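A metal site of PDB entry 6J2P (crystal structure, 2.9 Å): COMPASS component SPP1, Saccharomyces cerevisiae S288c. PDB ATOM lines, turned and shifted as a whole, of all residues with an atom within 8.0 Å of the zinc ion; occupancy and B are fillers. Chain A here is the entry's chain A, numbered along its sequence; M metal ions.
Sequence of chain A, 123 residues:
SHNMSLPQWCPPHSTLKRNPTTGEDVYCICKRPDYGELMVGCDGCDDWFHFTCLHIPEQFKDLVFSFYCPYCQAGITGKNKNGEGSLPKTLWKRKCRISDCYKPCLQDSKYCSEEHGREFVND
The nearest printed residue that does not touch the zinc ion is Arg 32 (4.6 Å).
The zinc ion is bound by a ring nitrogen (ND1) of His 50, the side-chain sulfur of Cys 30, the side-chain sulfur of Cys 53 and the side-chain sulfur of Cys 28. The zinc ion has four donor atoms within binding distance.
The backbone carbonyl oxygen of Trp 48 sits at hydrogen-bond distance from the backbone NH of Cys 28. A ring nitrogen (NE2) of His 50 sits close to the side-chain sulfur (SD) of Met 39. The side-chain sulfur of Cys 30 sits close to the backbone NH of Arg 32 (3.6 Å).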
ATOM      1  N   TYR A  27      -2.384  21.859  27.851  1.00  0.00           N
ATOM      2  CA  TYR A  27      -1.533  22.808  28.563  1.00  0.00           C
ATOM      3  C   TYR A  27      -1.685  24.183  27.928  1.00  0.00           C
ATOM      4  O   TYR A  27      -2.414  24.360  26.956  1.00  0.00           O
ATOM      5  CB  TYR A  27      -0.066  22.358  28.534  1.00  0.00           C
ATOM      6  CG  TYR A  27       0.176  20.978  29.101  1.00  0.00           C
ATOM      7  CD1 TYR A  27       0.156  19.863  28.278  1.00  0.00           C
ATOM      8  CD2 TYR A  27       0.445  20.799  30.452  1.00  0.00           C
ATOM      9  CE1 TYR A  27       0.382  18.592  28.790  1.00  0.00           C
ATOM     10  CE2 TYR A  27       0.677  19.536  30.959  1.00  0.00           C
ATOM     11  CZ  TYR A  27       0.647  18.442  30.134  1.00  0.00           C
ATOM     12  OH  TYR A  27       0.874  17.186  30.646  1.00  0.00           O
ATOM     13  N   CYS A  28      -0.973  25.155  28.497  1.00  0.00           N
ATOM     14  CA  CYS A  28      -0.814  26.481  27.899  1.00  0.00           C
ATOM     15  C   CYS A  28      -2.121  27.261  27.831  1.00  0.00           C
ATOM     16  O   CYS A  28      -3.162  26.795  28.296  1.00  0.00           O
ATOM     17  CB  CYS A  28      -0.211  26.347  26.492  1.00  0.00           C
ATOM     18  SG  CYS A  28       0.383  27.882  25.750  1.00  0.00           S
ATOM     19  N   ILE A  29      -2.058  28.480  27.282  1.00  0.00           N
ATOM     20  CA  ILE A  29      -3.267  29.277  27.100  1.00  0.00           C
ATOM     21  C   ILE A  29      -4.095  28.766  25.926  1.00  0.00           C
ATOM     22  O   ILE A  29      -5.307  29.041  25.866  1.00  0.00           O
ATOM     23  CB  ILE A  29      -2.908  30.758  26.878  1.00  0.00           C
ATOM     24  CG1 ILE A  29      -1.715  30.893  25.940  1.00  0.00           C
ATOM     25  CG2 ILE A  29      -2.635  31.439  28.211  1.00  0.00           C
ATOM     26  CD1 ILE A  29      -1.442  32.311  25.492  1.00  0.00           C
ATOM     27  N   CYS A  30      -3.473  28.054  24.982  1.00  0.00           N
ATOM     28  CA  CYS A  30      -4.196  27.440  23.877  1.00  0.00           C
ATOM     29  C   CYS A  30      -4.994  26.216  24.296  1.00  0.00           C
ATOM     30  O   CYS A  30      -5.923  25.821  23.580  1.00  0.00           O
ATOM     31  CB  CYS A  30      -3.208  27.044  22.769  1.00  0.00           C
ATOM     32  SG  CYS A  30      -1.948  25.827  23.294  1.00  0.00           S
ATOM     33  N   LYS A  31      -4.662  25.620  25.436  1.00  0.00           N
ATOM     34  CA  LYS A  31      -5.315  24.410  25.928  1.00  0.00           C
ATOM     35  C   LYS A  31      -5.295  23.306  24.866  1.00  0.00           C
ATOM     36  O   LYS A  31      -6.296  22.662  24.569  1.00  0.00           O
ATOM     37  CB  LYS A  31      -6.740  24.721  26.419  1.00  0.00           C
ATOM     38  CG  LYS A  31      -6.766  25.819  27.486  1.00  0.00           C
ATOM     39  CD  LYS A  31      -6.559  25.316  28.913  1.00  0.00           C
ATOM     40  CE  LYS A  31      -7.171  23.941  29.146  1.00  0.00           C
ATOM     41  NZ  LYS A  31      -6.708  23.300  30.432  1.00  0.00           N
ATOM     42  N   ARG A  32      -4.111  23.125  24.283  1.00  0.00           N
ATOM     43  CA  ARG A  32      -3.791  22.048  23.357  1.00  0.00           C
ATOM     44  C   ARG A  32      -2.793  21.091  24.000  1.00  0.00           C
ATOM     45  O   ARG A  32      -2.061  21.469  24.921  1.00  0.00           O
ATOM     46  CB  ARG A  32      -3.194  22.613  22.059  1.00  0.00           C
ATOM     47  CG  ARG A  32      -4.207  23.330  21.174  1.00  0.00           C
ATOM     48  CD  ARG A  32      -3.528  24.304  20.212  1.00  0.00           C
ATOM     49  NE  ARG A  32      -2.099  24.045  20.088  1.00  0.00           N
ATOM     50  CZ  ARG A  32      -1.217  24.930  19.624  1.00  0.00           C
ATOM     51  NH1 ARG A  32      -1.625  26.133  19.244  1.00  0.00           N
ATOM     52  NH2 ARG A  32       0.067  24.618  19.545  1.00  0.00           N
ATOM     53  N   PRO A  33      -2.730  19.843  23.548  1.00  0.00           N
ATOM     54  CA  PRO A  33      -1.851  18.855  24.188  1.00  0.00           C
ATOM     55  C   PRO A  33      -0.381  19.137  23.909  1.00  0.00           C
ATOM     56  O   PRO A  33      -0.015  19.956  23.066  1.00  0.00           O
ATOM     57  CB  PRO A  33      -2.287  17.519  23.585  1.00  0.00           C
ATOM     58  CG  PRO A  33      -3.621  17.785  22.984  1.00  0.00           C
ATOM     59  CD  PRO A  33      -3.603  19.210  22.552  1.00  0.00           C
ATOM     60  N   LEU A  38       8.516  22.943  21.867  1.00  0.00           N
ATOM     61  CA  LEU A  38       9.248  23.514  22.986  1.00  0.00           C
ATOM     62  C   LEU A  38       8.326  24.315  23.900  1.00  0.00           C
ATOM     63  O   LEU A  38       7.482  25.083  23.437  1.00  0.00           O
ATOM     64  CB  LEU A  38      10.394  24.378  22.455  1.00  0.00           C
ATOM     65  CG  LEU A  38      11.064  25.408  23.341  1.00  0.00           C
ATOM     66  CD1 LEU A  38      12.144  24.764  24.201  1.00  0.00           C
ATOM     67  CD2 LEU A  38      11.666  26.513  22.476  1.00  0.00           C
ATOM     68  N   MET A  39       8.510  24.152  25.209  1.00  0.00           N
ATOM     69  CA  MET A  39       7.622  24.743  26.205  1.00  0.00           C
ATOM     70  C   MET A  39       8.405  25.170  27.439  1.00  0.00           C
ATOM     71  O   MET A  39       9.520  24.706  27.688  1.00  0.00           O
ATOM     72  CB  MET A  39       6.510  23.766  26.612  1.00  0.00           C
ATOM     73  CG  MET A  39       5.381  23.651  25.620  1.00  0.00           C
ATOM     74  SD  MET A  39       4.051  22.573  26.214  1.00  0.00           S
ATOM     75  CE  MET A  39       4.894  20.997  26.224  1.00  0.00           C
ATOM     76  N   TRP A  48       2.317  24.392  31.728  1.00  0.00           N
ATOM     77  CA  TRP A  48       3.345  24.452  30.688  1.00  0.00           C
ATOM     78  C   TRP A  48       2.791  25.204  29.496  1.00  0.00           C
ATOM     79  O   TRP A  48       1.624  25.050  29.145  1.00  0.00           O
ATOM     80  CB  TRP A  48       3.799  23.049  30.284  1.00  0.00           C
ATOM     81  CG  TRP A  48       4.526  22.342  31.391  1.00  0.00           C
ATOM     82  CD1 TRP A  48       3.961  21.689  32.447  1.00  0.00           C
ATOM     83  CD2 TRP A  48       5.944  22.224  31.551  1.00  0.00           C
ATOM     84  NE1 TRP A  48       4.951  21.176  33.253  1.00  0.00           N
ATOM     85  CE2 TRP A  48       6.176  21.486  32.726  1.00  0.00           C
ATOM     86  CE3 TRP A  48       7.036  22.681  30.808  1.00  0.00           C
ATOM     87  CZ2 TRP A  48       7.460  21.193  33.179  1.00  0.00           C
ATOM     88  CZ3 TRP A  48       8.314  22.381  31.266  1.00  0.00           C
ATOM     89  CH2 TRP A  48       8.505  21.646  32.438  1.00  0.00           C
ATOM     90  N   PHE A  49       3.642  26.024  28.876  1.00  0.00           N
ATOM     91  CA  PHE A  49       3.212  26.959  27.849  1.00  0.00           C
ATOM     92  C   PHE A  49       4.133  26.898  26.649  1.00  0.00           C
ATOM     93  O   PHE A  49       5.360  26.881  26.804  1.00  0.00           O
ATOM     94  CB  PHE A  49       3.147  28.396  28.403  1.00  0.00           C
ATOM     95  CG  PHE A  49       2.231  28.535  29.594  1.00  0.00           C
ATOM     96  CD1 PHE A  49       0.938  28.976  29.436  1.00  0.00           C
ATOM     97  CD2 PHE A  49       2.685  28.222  30.871  1.00  0.00           C
ATOM     98  CE1 PHE A  49       0.089  29.106  30.524  1.00  0.00           C
ATOM     99  CE2 PHE A  49       1.847  28.344  31.961  1.00  0.00           C
ATOM    100  CZ  PHE A  49       0.548  28.785  31.795  1.00  0.00           C
ATOM    101  N   HIS A  50       3.551  26.871  25.452  1.00  0.00           N
ATOM    102  CA  HIS A  50       4.338  26.836  24.228  1.00  0.00           C
ATOM    103  C   HIS A  50       5.052  28.160  24.005  1.00  0.00           C
ATOM    104  O   HIS A  50       4.523  29.232  24.306  1.00  0.00           O
ATOM    105  CB  HIS A  50       3.441  26.530  23.030  1.00  0.00           C
ATOM    106  CG  HIS A  50       2.713  25.226  23.132  1.00  0.00           C
ATOM    107  ND1 HIS A  50       1.359  25.142  23.326  1.00  0.00           N
ATOM    108  CD2 HIS A  50       3.168  23.947  23.067  1.00  0.00           C
ATOM    109  CE1 HIS A  50       0.995  23.865  23.384  1.00  0.00           C
ATOM    110  NE2 HIS A  50       2.077  23.125  23.226  1.00  0.00           N
ATOM    111  N   PHE A  51       6.281  28.072  23.486  1.00  0.00           N
ATOM    112  CA  PHE A  51       6.999  29.280  23.097  1.00  0.00           C
ATOM    113  C   PHE A  51       6.219  30.082  22.062  1.00  0.00           C
ATOM    114  O   PHE A  51       6.094  31.310  22.187  1.00  0.00           O
ATOM    115  CB  PHE A  51       8.370  28.912  22.540  1.00  0.00           C
ATOM    116  CG  PHE A  51       9.485  28.986  23.540  1.00  0.00           C
ATOM    117  CD1 PHE A  51      10.528  29.875  23.377  1.00  0.00           C
ATOM    118  CD2 PHE A  51       9.501  28.147  24.644  1.00  0.00           C
ATOM    119  CE1 PHE A  51      11.562  29.944  24.289  1.00  0.00           C
ATOM    120  CE2 PHE A  51      10.537  28.194  25.550  1.00  0.00           C
ATOM    121  CZ  PHE A  51      11.565  29.100  25.390  1.00  0.00           C
ATOM    122  N   THR A  52       5.684  29.399  21.051  1.00  0.00           N
ATOM    123  CA  THR A  52       4.982  30.089  19.973  1.00  0.00           C
ATOM    124  C   THR A  52       3.726  30.797  20.476  1.00  0.00           C
ATOM    125  O   THR A  52       3.366  31.866  19.957  1.00  0.00           O
ATOM    126  CB  THR A  52       4.615  29.097  18.869  1.00  0.00           C
ATOM    127  OG1 THR A  52       3.972  27.961  19.441  1.00  0.00           O
ATOM    128  CG2 THR A  52       5.868  28.637  18.138  1.00  0.00           C
ATOM    129  N   CYS A  53       3.057  30.232  21.487  1.00  0.00           N
ATOM    130  CA  CYS A  53       1.857  30.878  22.014  1.00  0.00           C
ATOM    131  C   CYS A  53       2.206  32.137  22.810  1.00  0.00           C
ATOM    132  O   CYS A  53       1.389  33.070  22.869  1.00  0.00           O
ATOM    133  CB  CYS A  53       1.079  29.901  22.890  1.00  0.00           C
ATOM    134  SG  CYS A  53       0.319  28.539  21.968  1.00  0.00           S
ATOM    135  N   LEU A  54       3.390  32.188  23.406  1.00  0.00           N
ATOM    136  CA  LEU A  54       3.841  33.363  24.140  1.00  0.00           C
ATOM    137  C   LEU A  54       4.608  34.348  23.262  1.00  0.00           C
ATOM    138  O   LEU A  54       5.048  35.388  23.761  1.00  0.00           O
ATOM    139  CB  LEU A  54       4.740  32.938  25.311  1.00  0.00           C
ATOM    140  CG  LEU A  54       4.137  31.887  26.236  1.00  0.00           C
ATOM    141  CD1 LEU A  54       5.235  31.147  26.974  1.00  0.00           C
ATOM    142  CD2 LEU A  54       3.159  32.543  27.213  1.00  0.00           C
HETATM  143 ZN    ZN M   1       0.151  26.813  23.564  1.00  0.00          ZN
